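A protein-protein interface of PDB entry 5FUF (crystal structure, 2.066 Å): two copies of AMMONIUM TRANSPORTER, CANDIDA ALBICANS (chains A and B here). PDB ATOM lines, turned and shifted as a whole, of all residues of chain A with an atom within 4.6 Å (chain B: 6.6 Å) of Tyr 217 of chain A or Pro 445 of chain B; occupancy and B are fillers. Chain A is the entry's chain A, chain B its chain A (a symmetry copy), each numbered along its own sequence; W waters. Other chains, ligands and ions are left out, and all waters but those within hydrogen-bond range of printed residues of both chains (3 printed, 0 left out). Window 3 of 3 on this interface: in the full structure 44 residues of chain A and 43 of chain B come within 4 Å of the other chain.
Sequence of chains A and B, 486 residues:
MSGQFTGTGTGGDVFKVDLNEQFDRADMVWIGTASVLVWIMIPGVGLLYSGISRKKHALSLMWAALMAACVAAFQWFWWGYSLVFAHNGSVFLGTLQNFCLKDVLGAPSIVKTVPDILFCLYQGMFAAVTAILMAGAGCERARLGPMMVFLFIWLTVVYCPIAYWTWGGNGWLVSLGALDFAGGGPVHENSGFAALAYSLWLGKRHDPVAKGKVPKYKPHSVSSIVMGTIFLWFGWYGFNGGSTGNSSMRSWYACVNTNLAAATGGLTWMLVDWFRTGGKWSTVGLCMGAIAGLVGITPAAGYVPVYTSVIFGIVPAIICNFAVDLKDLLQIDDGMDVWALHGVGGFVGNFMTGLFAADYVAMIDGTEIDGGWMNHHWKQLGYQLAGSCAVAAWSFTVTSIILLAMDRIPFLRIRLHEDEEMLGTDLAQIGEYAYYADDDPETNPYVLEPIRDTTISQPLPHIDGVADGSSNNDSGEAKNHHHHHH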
ATOM      1  N   PRO A 215      16.819   4.834  20.145  1.00  0.00           N
ATOM      2  CA  PRO A 215      16.185   3.726  19.419  1.00  0.00           C
ATOM      3  C   PRO A 215      17.062   2.482  19.425  1.00  0.00           C
ATOM      4  O   PRO A 215      18.274   2.546  19.193  1.00  0.00           O
ATOM      5  CB  PRO A 215      15.987   4.290  18.003  1.00  0.00           C
ATOM      6  CG  PRO A 215      16.894   5.483  17.920  1.00  0.00           C
ATOM      7  CD  PRO A 215      16.968   6.035  19.304  1.00  0.00           C
ATOM      8  N   LYS A 216      16.436   1.348  19.749  1.00  0.00           N
ATOM      9  CA  LYS A 216      17.113   0.054  19.683  1.00  0.00           C
ATOM     10  C   LYS A 216      17.556  -0.280  18.259  1.00  0.00           C
ATOM     11  O   LYS A 216      18.656  -0.809  18.046  1.00  0.00           O
ATOM     12  CB  LYS A 216      16.178  -1.023  20.242  1.00  0.00           C
ATOM     13  CG  LYS A 216      16.707  -2.452  20.180  1.00  0.00           C
ATOM     14  CD  LYS A 216      15.793  -3.378  20.986  1.00  0.00           C
ATOM     15  CE  LYS A 216      16.264  -4.821  20.946  1.00  0.00           C
ATOM     16  NZ  LYS A 216      15.449  -5.655  21.890  1.00  0.00           N
ATOM     17  N   TYR A 217      16.727   0.026  17.272  1.00  0.00           N
ATOM     18  CA  TYR A 217      17.067  -0.166  15.866  1.00  0.00           C
ATOM     19  C   TYR A 217      17.190   1.195  15.193  1.00  0.00           C
ATOM     20  O   TYR A 217      16.259   2.003  15.257  1.00  0.00           O
ATOM     21  CB  TYR A 217      16.004  -1.009  15.151  1.00  0.00           C
ATOM     22  CG  TYR A 217      15.622  -2.261  15.908  1.00  0.00           C
ATOM     23  CD1 TYR A 217      16.538  -3.297  16.078  1.00  0.00           C
ATOM     24  CD2 TYR A 217      14.349  -2.417  16.440  1.00  0.00           C
ATOM     25  CE1 TYR A 217      16.202  -4.456  16.769  1.00  0.00           C
ATOM     26  CE2 TYR A 217      14.002  -3.566  17.138  1.00  0.00           C
ATOM     27  CZ  TYR A 217      14.930  -4.583  17.293  1.00  0.00           C
ATOM     28  OH  TYR A 217      14.596  -5.728  17.980  1.00  0.00           O
ATOM     29  N   LYS A 218      18.334   1.445  14.546  1.00  0.00           N
ATOM     30  CA  LYS A 218      18.549   2.681  13.789  1.00  0.00           C
ATOM     31  C   LYS A 218      19.484   2.373  12.623  1.00  0.00           C
ATOM     32  O   LYS A 218      20.640   2.812  12.589  1.00  0.00           O
ATOM     33  CB  LYS A 218      19.107   3.782  14.696  1.00  0.00           C
ATOM     34  CG  LYS A 218      19.210   5.169  14.070  1.00  0.00           C
ATOM     35  CD  LYS A 218      19.861   6.136  15.066  1.00  0.00           C
ATOM     36  CE  LYS A 218      20.771   7.144  14.376  1.00  0.00           C
ATOM     37  NZ  LYS A 218      21.910   7.558  15.270  1.00  0.00           N
ATOM     38  N   PRO A 219      19.000   1.623  11.632  1.00  0.00           N
ATOM     39  CA  PRO A 219      19.911   0.985  10.677  1.00  0.00           C
ATOM     40  C   PRO A 219      20.497   1.959   9.674  1.00  0.00           C
ATOM     41  O   PRO A 219      19.823   2.859   9.167  1.00  0.00           O
ATOM     42  CB  PRO A 219      19.020  -0.045   9.967  1.00  0.00           C
ATOM     43  CG  PRO A 219      17.649   0.547  10.046  1.00  0.00           C
ATOM     44  CD  PRO A 219      17.590   1.291  11.365  1.00  0.00           C
ATOM     45  N   TRP A 269      11.168 -13.227  16.512  1.00  0.00           N
ATOM     46  CA  TRP A 269      11.755 -11.928  16.848  1.00  0.00           C
ATOM     47  C   TRP A 269      10.814 -10.791  16.473  1.00  0.00           C
ATOM     48  O   TRP A 269      10.633  -9.842  17.246  1.00  0.00           O
ATOM     49  CB  TRP A 269      13.109 -11.755  16.151  1.00  0.00           C
ATOM     50  CG  TRP A 269      13.957 -10.565  16.607  1.00  0.00           C
ATOM     51  CD1 TRP A 269      13.599  -9.238  16.618  1.00  0.00           C
ATOM     52  CD2 TRP A 269      15.317 -10.612  17.074  1.00  0.00           C
ATOM     53  NE1 TRP A 269      14.649  -8.463  17.076  1.00  0.00           N
ATOM     54  CE2 TRP A 269      15.710  -9.281  17.363  1.00  0.00           C
ATOM     55  CE3 TRP A 269      16.243 -11.653  17.270  1.00  0.00           C
ATOM     56  CZ2 TRP A 269      16.986  -8.960  17.840  1.00  0.00           C
ATOM     57  CZ3 TRP A 269      17.507 -11.337  17.758  1.00  0.00           C
ATOM     58  CH2 TRP A 269      17.867  -9.991  18.033  1.00  0.00           C
ATOM     59  N   ASP A 273       9.104  -8.076  19.076  1.00  0.00           N
ATOM     60  CA  ASP A 273       9.138  -6.623  18.915  1.00  0.00           C
ATOM     61  C   ASP A 273       7.737  -6.044  18.759  1.00  0.00           C
ATOM     62  O   ASP A 273       7.490  -4.895  19.147  1.00  0.00           O
ATOM     63  CB  ASP A 273       9.988  -6.233  17.709  1.00  0.00           C
ATOM     64  CG  ASP A 273      11.479  -6.331  17.975  1.00  0.00           C
ATOM     65  OD1 ASP A 273      11.897  -6.502  19.131  1.00  0.00           O
ATOM     66  OD2 ASP A 273      12.244  -6.193  17.010  1.00  0.00           O
ATOM     67  N   TRP A 281       5.758  -3.407  13.357  1.00  0.00           N
ATOM     68  CA  TRP A 281       6.396  -4.525  12.674  1.00  0.00           C
ATOM     69  C   TRP A 281       7.840  -4.151  12.357  1.00  0.00           C
ATOM     70  O   TRP A 281       8.087  -3.263  11.537  1.00  0.00           O
ATOM     71  CB  TRP A 281       5.630  -4.888  11.401  1.00  0.00           C
ATOM     72  CG  TRP A 281       4.230  -5.363  11.663  1.00  0.00           C
ATOM     73  CD1 TRP A 281       3.060  -4.725  11.332  1.00  0.00           C
ATOM     74  CD2 TRP A 281       3.849  -6.578  12.321  1.00  0.00           C
ATOM     75  NE1 TRP A 281       1.979  -5.475  11.738  1.00  0.00           N
ATOM     76  CE2 TRP A 281       2.436  -6.615  12.351  1.00  0.00           C
ATOM     77  CE3 TRP A 281       4.567  -7.646  12.881  1.00  0.00           C
ATOM     78  CZ2 TRP A 281       1.727  -7.675  12.925  1.00  0.00           C
ATOM     79  CZ3 TRP A 281       3.863  -8.697  13.457  1.00  0.00           C
ATOM     80  CH2 TRP A 281       2.459  -8.707  13.469  1.00  0.00           C
ATOM     81  N   SER A 282       8.784  -4.831  12.998  1.00  0.00           N
ATOM     82  CA  SER A 282      10.203  -4.492  12.898  1.00  0.00           C
ATOM     83  C   SER A 282      10.812  -5.190  11.678  1.00  0.00           C
ATOM     84  O   SER A 282      10.925  -6.425  11.649  1.00  0.00           O
ATOM     85  CB  SER A 282      10.912  -4.893  14.192  1.00  0.00           C
ATOM     86  OG  SER A 282      12.288  -4.571  14.182  1.00  0.00           O
ATOM     87  N   THR A 283      11.207  -4.402  10.669  1.00  0.00           N
ATOM     88  CA  THR A 283      11.880  -4.982   9.505  1.00  0.00           C
ATOM     89  C   THR A 283      13.272  -5.485   9.876  1.00  0.00           C
ATOM     90  O   THR A 283      13.678  -6.575   9.453  1.00  0.00           O
ATOM     91  CB  THR A 283      11.978  -3.966   8.356  1.00  0.00           C
ATOM     92  OG1 THR A 283      12.595  -2.762   8.820  1.00  0.00           O
ATOM     93  CG2 THR A 283      10.586  -3.614   7.784  1.00  0.00           C
ATOM     94  N   VAL A 284      14.012  -4.707  10.671  1.00  0.00           N
ATOM     95  CA  VAL A 284      15.306  -5.164  11.177  1.00  0.00           C
ATOM     96  C   VAL A 284      15.125  -6.419  12.017  1.00  0.00           C
ATOM     97  O   VAL A 284      15.919  -7.369  11.924  1.00  0.00           O
ATOM     98  CB  VAL A 284      15.997  -4.044  11.979  1.00  0.00           C
ATOM     99  CG1 VAL A 284      17.346  -4.516  12.515  1.00  0.00           C
ATOM    100  CG2 VAL A 284      16.157  -2.774  11.100  1.00  0.00           C
ATOM    101  N   MET A 288      17.177 -10.110  11.952  1.00  0.00           N
ATOM    102  CA  MET A 288      17.975 -10.573  13.086  1.00  0.00           C
ATOM    103  C   MET A 288      17.441 -11.886  13.630  1.00  0.00           C
ATOM    104  O   MET A 288      18.221 -12.743  14.067  1.00  0.00           O
ATOM    105  CB  MET A 288      18.007  -9.517  14.200  1.00  0.00           C
ATOM    106  CG  MET A 288      18.646  -8.172  13.797  1.00  0.00           C
ATOM    107  SD  MET A 288      18.786  -7.009  15.181  1.00  0.00           S
ATOM    108  CE  MET A 288      20.171  -7.708  16.086  1.00  0.00           C
ATOM    109  N   ASN A 321      17.001 -11.394  21.350  1.00  0.00           N
ATOM    110  CA  ASN A 321      16.287 -10.119  21.328  1.00  0.00           C
ATOM    111  C   ASN A 321      16.532  -9.342  22.616  1.00  0.00           C
ATOM    112  O   ASN A 321      16.800  -8.133  22.588  1.00  0.00           O
ATOM    113  CB  ASN A 321      14.789 -10.361  21.104  1.00  0.00           C
ATOM    114  CG  ASN A 321      13.991  -9.059  20.961  1.00  0.00           C
ATOM    115  OD1 ASN A 321      14.013  -8.209  21.854  1.00  0.00           O
ATOM    116  ND2 ASN A 321      13.270  -8.915  19.846  1.00  0.00           N
ATOM    117  N   ASP B 440      11.549   7.015   4.644  1.00  0.00           N
ATOM    118  CA  ASP B 440      12.642   6.494   3.835  1.00  0.00           C
ATOM    119  C   ASP B 440      12.833   5.018   4.158  1.00  0.00           C
ATOM    120  O   ASP B 440      13.336   4.699   5.248  1.00  0.00           O
ATOM    121  CB  ASP B 440      13.929   7.284   4.114  1.00  0.00           C
ATOM    122  CG  ASP B 440      15.094   6.827   3.263  1.00  0.00           C
ATOM    123  OD1 ASP B 440      14.855   6.055   2.290  1.00  0.00           O
ATOM    124  OD2 ASP B 440      16.232   7.253   3.541  1.00  0.00           O
ATOM    125  N   PRO B 441      12.431   4.093   3.280  1.00  0.00           N
ATOM    126  CA  PRO B 441      12.535   2.675   3.615  1.00  0.00           C
ATOM    127  C   PRO B 441      13.969   2.211   3.816  1.00  0.00           C
ATOM    128  O   PRO B 441      14.188   1.145   4.404  1.00  0.00           O
ATOM    129  CB  PRO B 441      11.870   1.973   2.433  1.00  0.00           C
ATOM    130  CG  PRO B 441      11.763   2.996   1.354  1.00  0.00           C
ATOM    131  CD  PRO B 441      11.851   4.346   1.967  1.00  0.00           C
ATOM    132  N   THR B 443      16.142   3.570   5.820  1.00  0.00           N
ATOM    133  CA  THR B 443      16.567   3.791   7.197  1.00  0.00           C
ATOM    134  C   THR B 443      15.485   3.527   8.234  1.00  0.00           C
ATOM    135  O   THR B 443      15.807   3.425   9.420  1.00  0.00           O
ATOM    136  CB  THR B 443      17.075   5.236   7.382  1.00  0.00           C
ATOM    137  OG1 THR B 443      16.035   6.163   7.035  1.00  0.00           O
ATOM    138  CG2 THR B 443      18.303   5.489   6.513  1.00  0.00           C
ATOM    139  N   ASN B 444      14.229   3.427   7.832  1.00  0.00           N
ATOM    140  CA  ASN B 444      13.144   3.206   8.776  1.00  0.00           C
ATOM    141  C   ASN B 444      13.154   1.751   9.233  1.00  0.00           C
ATOM    142  O   ASN B 444      12.955   0.854   8.410  1.00  0.00           O
ATOM    143  CB  ASN B 444      11.813   3.562   8.123  1.00  0.00           C
ATOM    144  CG  ASN B 444      10.628   3.438   9.067  1.00  0.00           C
ATOM    145  OD1 ASN B 444      10.761   3.063  10.236  1.00  0.00           O
ATOM    146  ND2 ASN B 444       9.448   3.756   8.548  1.00  0.00           N
ATOM    147  N   PRO B 445      13.371   1.476  10.522  1.00  0.00           N
ATOM    148  CA  PRO B 445      13.385   0.087  11.001  1.00  0.00           C
ATOM    149  C   PRO B 445      12.008  -0.535  11.174  1.00  0.00           C
ATOM    150  O   PRO B 445      11.922  -1.709  11.553  1.00  0.00           O
ATOM    151  CB  PRO B 445      14.105   0.205  12.350  1.00  0.00           C
ATOM    152  CG  PRO B 445      13.730   1.585  12.837  1.00  0.00           C
ATOM    153  CD  PRO B 445      13.624   2.448  11.605  1.00  0.00           C
ATOM    154  N   TYR B 446      10.926   0.189  10.903  1.00  0.00           N
ATOM    155  CA  TYR B 446       9.584  -0.353  11.066  1.00  0.00           C
ATOM    156  C   TYR B 446       8.826  -0.274   9.751  1.00  0.00           C
ATOM    157  O   TYR B 446       9.045   0.632   8.939  1.00  0.00           O
ATOM    158  CB  TYR B 446       8.801   0.385  12.188  1.00  0.00           C
ATOM    159  CG  TYR B 446       9.514   0.304  13.521  1.00  0.00           C
ATOM    160  CD1 TYR B 446       9.588  -0.903  14.221  1.00  0.00           C
ATOM    161  CD2 TYR B 446      10.154   1.418  14.057  1.00  0.00           C
ATOM    162  CE1 TYR B 446      10.263  -0.992  15.431  1.00  0.00           C
ATOM    163  CE2 TYR B 446      10.830   1.342  15.268  1.00  0.00           C
ATOM    164  CZ  TYR B 446      10.884   0.135  15.949  1.00  0.00           C
ATOM    165  OH  TYR B 446      11.562   0.059  17.145  1.00  0.00           O
ATOM    166  N   VAL B 447       7.940  -1.256   9.547  1.00  0.00           N
ATOM    167  CA  VAL B 447       7.035  -1.237   8.406  1.00  0.00           C
ATOM    168  C   VAL B 447       6.158   0.006   8.487  1.00  0.00           C
ATOM    169  O   VAL B 447       5.615   0.332   9.547  1.00  0.00           O
ATOM    170  CB  VAL B 447       6.188  -2.519   8.380  1.00  0.00           C
ATOM    171  CG1 VAL B 447       5.106  -2.439   7.298  1.00  0.00           C
ATOM    172  CG2 VAL B 447       7.074  -3.730   8.141  1.00  0.00           C
HETATM  173  O   HOH W   1      12.247  -0.391   6.333  1.00  0.00           O
HETATM  174  O   HOH W   2       4.995  -1.072  11.867  1.00  0.00           O
HETATM  175  O   HOH W   3      13.808   1.300  17.383  1.00  0.00           O
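Printed residues of chain A that touch a printed residue of chain B: Tyr 217, Pro 219, Trp 281, Ser 282, Thr 283 and Val 284.
Of the 7 printed residues of chain B, 5 touch a printed residue of chain A.
Among the printed residues, no Asp or Glu carboxylate lies within 4 Å of a Lys or Arg side-chain nitrogen of the other chain.
The side-chain hydroxyl (OH) of Tyr 217 of chain A lies within hydrogen-bond range of the indole nitrogen (NE1) of Trp 269 of chain A (2.9 Å).
OH of Tyr 217 of chain A is in hydrogen-bond range of OD2 of Asp 273 of chain A (2.6 Å).
The side-chain carboxylate of Asp 273 of chain A is in hydrogen-bond range of the side-chain hydroxyl of Ser 282 of chain A.
The side-chain amide oxygen of Asn 444 of chain B is in hydrogen-bond range of the backbone NH of Tyr 446 of chain B (3.0 Å).
Among the printed residues, merely in contact across the chains: Tyr 217 of chain A with Pro 445 of chain B, Tyr 217 of chain A with Tyr 446 of chain B, Pro 219 of chain A with Thr 443 of chain B, Pro 219 of chain A with Pro 445 of chain B, Trp 281 of chain A with Tyr 446 of chain B, Ser 282 of chain A with Pro 445 of chain B, Ser 282 of chain A with Tyr 446 of chain B, Thr 283 of chain A with Asn 444 of chain B, Thr 283 of chain A with Tyr 446 of chain B, Thr 283 of chain A with Val 447 of chain B and Val 284 of chain A with Pro 445 of chain B.
No position is printed for both chains.
Of the 13 pairs that touch across the chains among the printed residues, none has its exchanged pair printed and touching as well.
Water W1 lies within hydrogen-bond range of the backbone carbonyl oxygen (O) of Asn 444 of chain B, the backbone carbonyl oxygen (O) of Pro 441 of chain B and the side-chain hydroxyl (OG1) of Thr 283 of chain A.
Water W3 lies within hydrogen-bond range of the side-chain hydroxyl of Tyr 446 of chain B and the backbone NH of Tyr 217 of chain A.
Water W2 bridges the backbone carbonyl oxygen (O) of Val 447 of chain B (2.8 Å) and the backbone NH (N) of Trp 281 of chain A (2.9 Å).
O of Trp 281 of chain A is in hydrogen-bond range of N of Val 447 of chain B, at 2.8 Å.
The backbone carbonyl oxygen of Pro 445 of chain B is in hydrogen-bond range of the backbone NH of Thr 283 of chain A, at 2.9 Å.
Lys 216 of chain A touches none of the printed residues of chain B.
Of chain B, only Pro 445 (3.5 Å) and Tyr 446 (3.8 Å) come within 4 Å of Tyr 217 of chain A.
Trp 269 of chain A touches none of the printed residues of chain B.
Printed residues of chain B within 4 Å of Trp 281 of chain A: Tyr 446 and Val 447.
Of the printed residues of chain A, Pro 445 of chain B touches Tyr 217 (3.5 Å), Pro 219 (3.8 Å), Ser 282 (3.5 Å), Thr 283 (2.9 Å) and Val 284 (3.8 Å).
Printed residues of chain A within 4 Å of Tyr 446 of chain B: Tyr 217, Trp 281, Ser 282 and Thr 283.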
